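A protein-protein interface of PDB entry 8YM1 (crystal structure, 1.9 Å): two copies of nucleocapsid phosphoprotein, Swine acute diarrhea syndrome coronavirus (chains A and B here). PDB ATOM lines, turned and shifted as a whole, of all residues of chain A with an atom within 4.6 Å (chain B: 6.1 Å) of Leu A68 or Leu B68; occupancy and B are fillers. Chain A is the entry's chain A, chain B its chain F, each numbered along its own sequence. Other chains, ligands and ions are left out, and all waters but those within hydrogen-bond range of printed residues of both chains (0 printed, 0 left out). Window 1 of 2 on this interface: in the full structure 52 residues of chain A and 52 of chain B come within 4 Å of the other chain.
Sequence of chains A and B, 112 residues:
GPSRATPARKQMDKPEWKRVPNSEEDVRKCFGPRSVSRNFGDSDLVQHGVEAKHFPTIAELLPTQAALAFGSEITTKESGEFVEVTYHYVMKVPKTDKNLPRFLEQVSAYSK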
ATOM      1  N   PRO A  63       8.403   1.834  28.856  1.00  0.00           N
ATOM      2  CA  PRO A  63       8.614   3.129  29.487  1.00  0.00           C
ATOM      3  C   PRO A  63       7.308   3.887  29.688  1.00  0.00           C
ATOM      4  O   PRO A  63       6.324   3.635  28.986  1.00  0.00           O
ATOM      5  CB  PRO A  63       9.560   3.845  28.501  1.00  0.00           C
ATOM      6  CG  PRO A  63       9.187   3.257  27.153  1.00  0.00           C
ATOM      7  CD  PRO A  63       8.842   1.804  27.453  1.00  0.00           C
ATOM      8  N   THR A  64       7.287   4.761  30.702  1.00  0.00           N
ATOM      9  CA  THR A  64       6.162   5.656  30.909  1.00  0.00           C
ATOM     10  C   THR A  64       6.163   6.672  29.775  1.00  0.00           C
ATOM     11  O   THR A  64       7.160   6.806  29.060  1.00  0.00           O
ATOM     12  CB  THR A  64       6.252   6.334  32.279  1.00  0.00           C
ATOM     13  OG1 THR A  64       7.504   7.012  32.299  1.00  0.00           O
ATOM     14  CG2 THR A  64       6.165   5.348  33.429  1.00  0.00           C
ATOM     15  N   GLN A  65       5.052   7.387  29.624  1.00  0.00           N
ATOM     16  CA  GLN A  65       4.913   8.369  28.561  1.00  0.00           C
ATOM     17  C   GLN A  65       5.952   9.483  28.759  1.00  0.00           C
ATOM     18  O   GLN A  65       6.547   9.958  27.792  1.00  0.00           O
ATOM     19  CB  GLN A  65       3.487   8.915  28.538  1.00  0.00           C
ATOM     20  CG  GLN A  65       3.128   9.656  27.256  1.00  0.00           C
ATOM     21  CD  GLN A  65       1.719  10.206  27.268  1.00  0.00           C
ATOM     22  OE1 GLN A  65       1.373  11.070  28.079  1.00  0.00           O
ATOM     23  NE2 GLN A  65       0.891   9.710  26.359  1.00  0.00           N
ATOM     24  N   ALA A  66       6.211   9.833  30.034  1.00  0.00           N
ATOM     25  CA  ALA A  66       7.169  10.879  30.380  1.00  0.00           C
ATOM     26  C   ALA A  66       8.604  10.399  30.131  1.00  0.00           C
ATOM     27  O   ALA A  66       9.452  11.181  29.704  1.00  0.00           O
ATOM     28  CB  ALA A  66       6.973  11.300  31.819  1.00  0.00           C
ATOM     29  N   ALA A  67       8.876   9.121  30.459  1.00  0.00           N
ATOM     30  CA  ALA A  67      10.198   8.533  30.256  1.00  0.00           C
ATOM     31  C   ALA A  67      10.530   8.491  28.767  1.00  0.00           C
ATOM     32  O   ALA A  67      11.668   8.744  28.374  1.00  0.00           O
ATOM     33  CB  ALA A  67      10.259   7.153  30.876  1.00  0.00           C
ATOM     34  N   LEU A  68       9.524   8.153  27.949  1.00  0.00           N
ATOM     35  CA  LEU A  68       9.677   8.127  26.504  1.00  0.00           C
ATOM     36  C   LEU A  68      10.006   9.535  26.005  1.00  0.00           C
ATOM     37  O   LEU A  68      10.902   9.711  25.192  1.00  0.00           O
ATOM     38  CB  LEU A  68       8.395   7.597  25.859  1.00  0.00           C
ATOM     39  CG  LEU A  68       8.402   7.489  24.330  1.00  0.00           C
ATOM     40  CD1 LEU A  68       9.384   6.435  23.846  1.00  0.00           C
ATOM     41  CD2 LEU A  68       7.019   7.203  23.809  1.00  0.00           C
ATOM     42  N   ALA A  69       9.290  10.531  26.543  1.00  0.00           N
ATOM     43  CA  ALA A  69       9.429  11.915  26.112  1.00  0.00           C
ATOM     44  C   ALA A  69      10.834  12.454  26.415  1.00  0.00           C
ATOM     45  O   ALA A  69      11.512  12.944  25.517  1.00  0.00           O
ATOM     46  CB  ALA A  69       8.361  12.766  26.778  1.00  0.00           C
ATOM     47  N   PHE A  70      11.290  12.272  27.666  1.00  0.00           N
ATOM     48  CA  PHE A  70      12.515  12.911  28.152  1.00  0.00           C
ATOM     49  C   PHE A  70      13.741  11.995  28.021  1.00  0.00           C
ATOM     50  O   PHE A  70      14.855  12.422  28.324  1.00  0.00           O
ATOM     51  CB  PHE A  70      12.283  13.313  29.613  1.00  0.00           C
ATOM     52  CG  PHE A  70      11.212  14.378  29.819  1.00  0.00           C
ATOM     53  CD1 PHE A  70      11.164  15.519  29.011  1.00  0.00           C
ATOM     54  CD2 PHE A  70      10.169  14.172  30.724  1.00  0.00           C
ATOM     55  CE1 PHE A  70      10.168  16.474  29.189  1.00  0.00           C
ATOM     56  CE2 PHE A  70       9.164  15.123  30.879  1.00  0.00           C
ATOM     57  CZ  PHE A  70       9.167  16.269  30.113  1.00  0.00           C
ATOM     58  N   GLY A  71      13.540  10.750  27.554  1.00  0.00           N
ATOM     59  CA  GLY A  71      14.638   9.788  27.451  1.00  0.00           C
ATOM     60  C   GLY A  71      14.912   9.350  26.007  1.00  0.00           C
ATOM     61  O   GLY A  71      15.829   8.566  25.770  1.00  0.00           O
ATOM     62  N   SER A  72      14.157   9.912  25.042  1.00  0.00           N
ATOM     63  CA  SER A  72      14.273   9.514  23.643  1.00  0.00           C
ATOM     64  C   SER A  72      15.008  10.571  22.838  1.00  0.00           C
ATOM     65  O   SER A  72      15.096  11.728  23.247  1.00  0.00           O
ATOM     66  CB  SER A  72      12.914   9.264  23.032  1.00  0.00           C
ATOM     67  OG  SER A  72      12.210   8.255  23.725  1.00  0.00           O
ATOM     68  N   TYR A  87      10.651   8.494  17.313  1.00  0.00           N
ATOM     69  CA  TYR A  87      11.161   8.319  18.666  1.00  0.00           C
ATOM     70  C   TYR A  87      12.179   7.184  18.669  1.00  0.00           C
ATOM     71  O   TYR A  87      11.894   6.092  18.180  1.00  0.00           O
ATOM     72  CB  TYR A  87      10.042   7.983  19.657  1.00  0.00           C
ATOM     73  CG  TYR A  87       9.011   9.077  19.880  1.00  0.00           C
ATOM     74  CD1 TYR A  87       7.969   9.268  18.980  1.00  0.00           C
ATOM     75  CD2 TYR A  87       8.967   9.784  21.081  1.00  0.00           C
ATOM     76  CE1 TYR A  87       6.986  10.220  19.205  1.00  0.00           C
ATOM     77  CE2 TYR A  87       7.983  10.732  21.325  1.00  0.00           C
ATOM     78  CZ  TYR A  87       6.990  10.951  20.382  1.00  0.00           C
ATOM     79  OH  TYR A  87       6.017  11.877  20.610  1.00  0.00           O
ATOM     80  N   TYR A  89      14.200   5.305  21.510  1.00  0.00           N
ATOM     81  CA  TYR A  89      14.337   5.134  22.947  1.00  0.00           C
ATOM     82  C   TYR A  89      15.145   3.877  23.241  1.00  0.00           C
ATOM     83  O   TYR A  89      14.826   2.802  22.741  1.00  0.00           O
ATOM     84  CB  TYR A  89      12.960   5.074  23.610  1.00  0.00           C
ATOM     85  CG  TYR A  89      13.024   4.986  25.123  1.00  0.00           C
ATOM     86  CD1 TYR A  89      13.274   6.115  25.893  1.00  0.00           C
ATOM     87  CD2 TYR A  89      12.819   3.782  25.786  1.00  0.00           C
ATOM     88  CE1 TYR A  89      13.372   6.044  27.272  1.00  0.00           C
ATOM     89  CE2 TYR A  89      12.895   3.697  27.169  1.00  0.00           C
ATOM     90  CZ  TYR A  89      13.174   4.833  27.914  1.00  0.00           C
ATOM     91  OH  TYR A  89      13.251   4.764  29.271  1.00  0.00           O
ATOM     92  N   TRP B  17      13.115   3.953  33.198  1.00  0.00           N
ATOM     93  CA  TRP B  17      12.031   3.924  32.214  1.00  0.00           C
ATOM     94  C   TRP B  17      10.645   4.065  32.878  1.00  0.00           C
ATOM     95  O   TRP B  17       9.661   4.282  32.180  1.00  0.00           O
ATOM     96  CB  TRP B  17      12.115   2.649  31.351  1.00  0.00           C
ATOM     97  CG  TRP B  17      12.002   1.356  32.117  1.00  0.00           C
ATOM     98  CD1 TRP B  17      10.862   0.656  32.382  1.00  0.00           C
ATOM     99  CD2 TRP B  17      13.090   0.564  32.640  1.00  0.00           C
ATOM    100  NE1 TRP B  17      11.157  -0.495  33.066  1.00  0.00           N
ATOM    101  CE2 TRP B  17      12.516  -0.584  33.232  1.00  0.00           C
ATOM    102  CE3 TRP B  17      14.486   0.712  32.668  1.00  0.00           C
ATOM    103  CZ2 TRP B  17      13.289  -1.568  33.848  1.00  0.00           C
ATOM    104  CZ3 TRP B  17      15.248  -0.264  33.276  1.00  0.00           C
ATOM    105  CH2 TRP B  17      14.656  -1.390  33.855  1.00  0.00           C
ATOM    106  N   PHE B  31      16.515  12.056  34.059  1.00  0.00           N
ATOM    107  CA  PHE B  31      17.023  11.594  32.757  1.00  0.00           C
ATOM    108  C   PHE B  31      18.306  12.321  32.332  1.00  0.00           C
ATOM    109  O   PHE B  31      18.789  12.102  31.219  1.00  0.00           O
ATOM    110  CB  PHE B  31      15.929  11.775  31.705  1.00  0.00           C
ATOM    111  CG  PHE B  31      14.663  11.001  32.010  1.00  0.00           C
ATOM    112  CD1 PHE B  31      14.585   9.636  31.746  1.00  0.00           C
ATOM    113  CD2 PHE B  31      13.542  11.634  32.537  1.00  0.00           C
ATOM    114  CE1 PHE B  31      13.440   8.922  32.055  1.00  0.00           C
ATOM    115  CE2 PHE B  31      12.393  10.912  32.821  1.00  0.00           C
ATOM    116  CZ  PHE B  31      12.352   9.560  32.598  1.00  0.00           C
ATOM    117  N   LEU B  62       2.106  12.490  22.418  1.00  0.00           N
ATOM    118  CA  LEU B  62       2.948  11.425  22.944  1.00  0.00           C
ATOM    119  C   LEU B  62       2.172  10.112  22.851  1.00  0.00           C
ATOM    120  O   LEU B  62       0.999  10.059  23.227  1.00  0.00           O
ATOM    121  CB  LEU B  62       3.370  11.725  24.385  1.00  0.00           C
ATOM    122  CG  LEU B  62       4.359  12.882  24.578  1.00  0.00           C
ATOM    123  CD1 LEU B  62       4.584  13.157  26.052  1.00  0.00           C
ATOM    124  CD2 LEU B  62       5.686  12.590  23.893  1.00  0.00           C
ATOM    125  N   PRO B  63       2.780   9.022  22.312  1.00  0.00           N
ATOM    126  CA  PRO B  63       2.080   7.746  22.184  1.00  0.00           C
ATOM    127  C   PRO B  63       1.824   7.081  23.531  1.00  0.00           C
ATOM    128  O   PRO B  63       2.539   7.336  24.503  1.00  0.00           O
ATOM    129  CB  PRO B  63       3.035   6.915  21.290  1.00  0.00           C
ATOM    130  CG  PRO B  63       4.401   7.487  21.593  1.00  0.00           C
ATOM    131  CD  PRO B  63       4.158   8.971  21.797  1.00  0.00           C
ATOM    132  N   THR B  64       0.771   6.252  23.586  1.00  0.00           N
ATOM    133  CA  THR B  64       0.463   5.482  24.778  1.00  0.00           C
ATOM    134  C   THR B  64       1.495   4.370  24.916  1.00  0.00           C
ATOM    135  O   THR B  64       2.241   4.085  23.976  1.00  0.00           O
ATOM    136  CB  THR B  64      -0.961   4.922  24.707  1.00  0.00           C
ATOM    137  OG1 THR B  64      -1.027   4.163  23.503  1.00  0.00           O
ATOM    138  CG2 THR B  64      -2.018   6.011  24.705  1.00  0.00           C
ATOM    139  N   GLN B  65       1.491   3.719  26.075  1.00  0.00           N
ATOM    140  CA  GLN B  65       2.433   2.655  26.370  1.00  0.00           C
ATOM    141  C   GLN B  65       2.191   1.481  25.411  1.00  0.00           C
ATOM    142  O   GLN B  65       3.139   0.916  24.868  1.00  0.00           O
ATOM    143  CB  GLN B  65       2.282   2.264  27.839  1.00  0.00           C
ATOM    144  CG  GLN B  65       3.402   1.384  28.368  1.00  0.00           C
ATOM    145  CD  GLN B  65       3.298   1.137  29.857  1.00  0.00           C
ATOM    146  OE1 GLN B  65       4.124   1.609  30.645  1.00  0.00           O
ATOM    147  NE2 GLN B  65       2.225   0.473  30.263  1.00  0.00           N
ATOM    148  N   ALA B  66       0.905   1.194  25.138  1.00  0.00           N
ATOM    149  CA  ALA B  66       0.519   0.103  24.251  1.00  0.00           C
ATOM    150  C   ALA B  66       0.877   0.440  22.799  1.00  0.00           C
ATOM    151  O   ALA B  66       1.326  -0.432  22.053  1.00  0.00           O
ATOM    152  CB  ALA B  66      -0.954  -0.181  24.401  1.00  0.00           C
ATOM    153  N   ALA B  67       0.635   1.701  22.400  1.00  0.00           N
ATOM    154  CA  ALA B  67       0.939   2.156  21.047  1.00  0.00           C
ATOM    155  C   ALA B  67       2.434   2.015  20.770  1.00  0.00           C
ATOM    156  O   ALA B  67       2.827   1.615  19.675  1.00  0.00           O
ATOM    157  CB  ALA B  67       0.470   3.584  20.855  1.00  0.00           C
ATOM    158  N   LEU B  68       3.258   2.337  21.781  1.00  0.00           N
ATOM    159  CA  LEU B  68       4.704   2.220  21.668  1.00  0.00           C
ATOM    160  C   LEU B  68       5.084   0.752  21.463  1.00  0.00           C
ATOM    161  O   LEU B  68       5.910   0.437  20.622  1.00  0.00           O
ATOM    162  CB  LEU B  68       5.376   2.789  22.918  1.00  0.00           C
ATOM    163  CG  LEU B  68       6.910   2.761  22.928  1.00  0.00           C
ATOM    164  CD1 LEU B  68       7.489   3.759  21.943  1.00  0.00           C
ATOM    165  CD2 LEU B  68       7.448   3.001  24.315  1.00  0.00           C
ATOM    166  N   ALA B  69       4.473  -0.132  22.260  1.00  0.00           N
ATOM    167  CA  ALA B  69       4.790  -1.553  22.229  1.00  0.00           C
ATOM    168  C   ALA B  69       4.417  -2.173  20.877  1.00  0.00           C
ATOM    169  O   ALA B  69       5.238  -2.845  20.260  1.00  0.00           O
ATOM    170  CB  ALA B  69       4.085  -2.258  23.367  1.00  0.00           C
ATOM    171  N   PHE B  70       3.203  -1.864  20.392  1.00  0.00           N
ATOM    172  CA  PHE B  70       2.637  -2.536  19.222  1.00  0.00           C
ATOM    173  C   PHE B  70       2.878  -1.743  17.928  1.00  0.00           C
ATOM    174  O   PHE B  70       2.609  -2.256  16.842  1.00  0.00           O
ATOM    175  CB  PHE B  70       1.144  -2.752  19.494  1.00  0.00           C
ATOM    176  CG  PHE B  70       0.842  -3.725  20.631  1.00  0.00           C
ATOM    177  CD1 PHE B  70       1.530  -4.939  20.737  1.00  0.00           C
ATOM    178  CD2 PHE B  70      -0.005  -3.358  21.680  1.00  0.00           C
ATOM    179  CE1 PHE B  70       1.276  -5.808  21.791  1.00  0.00           C
ATOM    180  CE2 PHE B  70      -0.236  -4.224  22.743  1.00  0.00           C
ATOM    181  CZ  PHE B  70       0.405  -5.445  22.795  1.00  0.00           C
ATOM    182  N   GLY B  71       3.412  -0.514  18.043  1.00  0.00           N
ATOM    183  CA  GLY B  71       3.631   0.336  16.873  1.00  0.00           C
ATOM    184  C   GLY B  71       5.119   0.587  16.587  1.00  0.00           C
ATOM    185  O   GLY B  71       5.449   1.262  15.614  1.00  0.00           O
ATOM    186  N   SER B  72       6.011  -0.013  17.404  1.00  0.00           N
ATOM    187  CA  SER B  72       7.450   0.223  17.286  1.00  0.00           C
ATOM    188  C   SER B  72       8.153  -0.985  16.688  1.00  0.00           C
ATOM    189  O   SER B  72       7.630  -2.098  16.718  1.00  0.00           O
ATOM    190  CB  SER B  72       8.067   0.549  18.633  1.00  0.00           C
ATOM    191  OG  SER B  72       7.433   1.656  19.247  1.00  0.00           O
ATOM    192  N   GLU B  73       9.340  -0.733  16.117  1.00  0.00           N
ATOM    193  CA  GLU B  73      10.282  -1.784  15.794  1.00  0.00           C
ATOM    194  C   GLU B  73      11.194  -1.939  17.005  1.00  0.00           C
ATOM    195  O   GLU B  73      11.903  -0.997  17.364  1.00  0.00           O
ATOM    196  CB  GLU B  73      11.111  -1.470  14.548  1.00  0.00           C
ATOM    197  CG  GLU B  73      12.159  -2.542  14.239  1.00  0.00           C
ATOM    198  CD  GLU B  73      13.020  -2.275  13.018  1.00  0.00           C
ATOM    199  OE1 GLU B  73      12.818  -1.240  12.351  1.00  0.00           O
ATOM    200  OE2 GLU B  73      13.923  -3.096  12.755  1.00  0.00           O
ATOM    201  N   ILE B  74      11.096  -3.086  17.684  1.00  0.00           N
ATOM    202  CA  ILE B  74      11.831  -3.308  18.918  1.00  0.00           C
ATOM    203  C   ILE B  74      12.954  -4.311  18.662  1.00  0.00           C
ATOM    204  O   ILE B  74      12.719  -5.398  18.135  1.00  0.00           O
ATOM    205  CB  ILE B  74      10.880  -3.757  20.045  1.00  0.00           C
ATOM    206  CG1 ILE B  74       9.755  -2.710  20.268  1.00  0.00           C
ATOM    207  CG2 ILE B  74      11.652  -4.046  21.341  1.00  0.00           C
ATOM    208  CD1 ILE B  74       8.760  -3.075  21.353  1.00  0.00           C
ATOM    209  N   TYR B  87      13.611   0.991  21.107  1.00  0.00           N
ATOM    210  CA  TYR B  87      12.305   1.207  20.503  1.00  0.00           C
ATOM    211  C   TYR B  87      12.449   2.230  19.383  1.00  0.00           C
ATOM    212  O   TYR B  87      13.056   3.280  19.582  1.00  0.00           O
ATOM    213  CB  TYR B  87      11.289   1.731  21.522  1.00  0.00           C
ATOM    214  CG  TYR B  87      10.976   0.792  22.673  1.00  0.00           C
ATOM    215  CD1 TYR B  87      11.801   0.734  23.789  1.00  0.00           C
ATOM    216  CD2 TYR B  87       9.775   0.088  22.717  1.00  0.00           C
ATOM    217  CE1 TYR B  87      11.496  -0.076  24.871  1.00  0.00           C
ATOM    218  CE2 TYR B  87       9.452  -0.719  23.798  1.00  0.00           C
ATOM    219  CZ  TYR B  87      10.317  -0.804  24.877  1.00  0.00           C
ATOM    220  OH  TYR B  87      10.011  -1.594  25.941  1.00  0.00           O
ATOM    221  N   HIS B  88      11.918   1.893  18.201  1.00  0.00           N
ATOM    222  CA  HIS B  88      11.888   2.811  17.073  1.00  0.00           C
ATOM    223  C   HIS B  88      10.431   3.021  16.678  1.00  0.00           C
ATOM    224  O   HIS B  88       9.819   2.140  16.077  1.00  0.00           O
ATOM    225  CB  HIS B  88      12.748   2.287  15.918  1.00  0.00           C
ATOM    226  CG  HIS B  88      12.867   3.244  14.778  1.00  0.00           C
ATOM    227  ND1 HIS B  88      11.980   3.273  13.723  1.00  0.00           N
ATOM    228  CD2 HIS B  88      13.754   4.223  14.541  1.00  0.00           C
ATOM    229  CE1 HIS B  88      12.333   4.234  12.881  1.00  0.00           C
ATOM    230  NE2 HIS B  88      13.405   4.823  13.356  1.00  0.00           N
ATOM    231  N   TYR B  89       9.865   4.167  17.095  1.00  0.00           N
ATOM    232  CA  TYR B  89       8.455   4.459  16.881  1.00  0.00           C
ATOM    233  C   TYR B  89       8.311   5.669  15.964  1.00  0.00           C
ATOM    234  O   TYR B  89       8.965   6.688  16.173  1.00  0.00           O
ATOM    235  CB  TYR B  89       7.764   4.705  18.222  1.00  0.00           C
ATOM    236  CG  TYR B  89       6.271   4.945  18.103  1.00  0.00           C
ATOM    237  CD1 TYR B  89       5.384   3.880  17.996  1.00  0.00           C
ATOM    238  CD2 TYR B  89       5.747   6.231  18.085  1.00  0.00           C
ATOM    239  CE1 TYR B  89       4.022   4.087  17.853  1.00  0.00           C
ATOM    240  CE2 TYR B  89       4.384   6.453  17.957  1.00  0.00           C
ATOM    241  CZ  TYR B  89       3.519   5.376  17.837  1.00  0.00           C
ATOM    242  OH  TYR B  89       2.183   5.577  17.707  1.00  0.00           O
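The side-chain amide nitrogen (NE2) of Gln A65 is in hydrogen-bond range of the backbone carbonyl oxygen (O) of Pro B63 (3.4 Å).
N of Thr A64 lies within hydrogen-bond range of O of Trp B17 (2.8 Å).
The backbone carbonyl oxygen (O) of Tyr B89 lies within hydrogen-bond range of the backbone NH (N) of Tyr A87 (2.7 Å).
N of Tyr B87 sits at hydrogen-bond distance from O of Tyr A89 (2.7 Å).
The side-chain amide nitrogen (NE2) of Gln A65 lies within hydrogen-bond range of the backbone carbonyl oxygen (O) of Leu B62 (3.2 Å).
The backbone carbonyl oxygen of Tyr A87 lies close to the backbone carbonyl oxygen of Tyr B87, 3.4 Å away.
O of Pro A63 lies close to OE1 of Gln B65 (3.4 Å).
Leu A68 touches just these residues of chain B: Pro B63 and Leu B68.
Of the printed residues of chain A, Leu B68 touches Pro A63 (3.3 Å) and Leu A68 (3.8 Å).
Printed residues of chain A within 4 Å of Tyr B89: Tyr A87.
Of the printed residues of chain A, Pro B63 touches Gln A65 (3.4 Å), Leu A68 (3.4 Å) and Tyr A87 (3.6 Å).
Of the printed residues of chain B, Thr A64 touches Trp B17 (2.8 Å).
Printed residues of chain B within 4 Å of Phe A70: Phe B31 (3.6 Å).
Of the printed residues of chain A, Trp B17 touches Pro A63 (3.1 Å), Thr A64 (2.8 Å), Ala A67 (3.2 Å) and Tyr A89 (3.2 Å).
Glu B73 touches none of the printed residues of chain A.
Ala A66 touches none of the printed residues of chain B.
Among the printed residues, no Asp or Glu carboxylate lies within 4 Å of a Lys or Arg side-chain nitrogen of the other chain.
Among the printed residues, pairs that only touch across the chains: Pro A63 with Trp B17 (3.1 Å), Pro A63 with Leu B68 (3.3 Å), Pro A63 with Tyr B87 (3.9 Å), Ala A67 with Trp B17 (3.2 Å), Ala A67 with Phe B31 (3.3 Å), Leu A68 with Pro B63 (3.4 Å), Leu A68 with Leu B68 (3.8 Å), Ala A69 with Leu B62 (3.9 Å), Phe A70 with Phe B31 (3.6 Å), Tyr A87 with Leu B62 (3.4 Å), Tyr A87 with Pro B63 (3.6 Å), Tyr A87 with His B88 (3.5 Å) and Tyr A89 with Trp B17 (3.2 Å).
N of Glu B73 sits at hydrogen-bond distance from O of His B88, 2.9 Å away.
OG1 of Thr A64 lies close to N of Ala A67, 3.1 Å away.
The backbone carbonyl oxygen (O) of Leu A68 lies within hydrogen-bond range of the side-chain hydroxyl (OG) of Ser A72.
Pro A63 touches Gln B65, and with the chains exchanged Gln A65 touches Pro B63.
Pro A63 touches Leu B68, and with the chains exchanged Leu A68 touches Pro B63.
Leu B68 touches its own counterpart, Leu A68.
Tyr A87 touches its own counterpart, Tyr B87.
Positions printed for both chains: 63, 64, 65, 66, 67, 68, 69, 70, 71, 72, 87 and 89.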
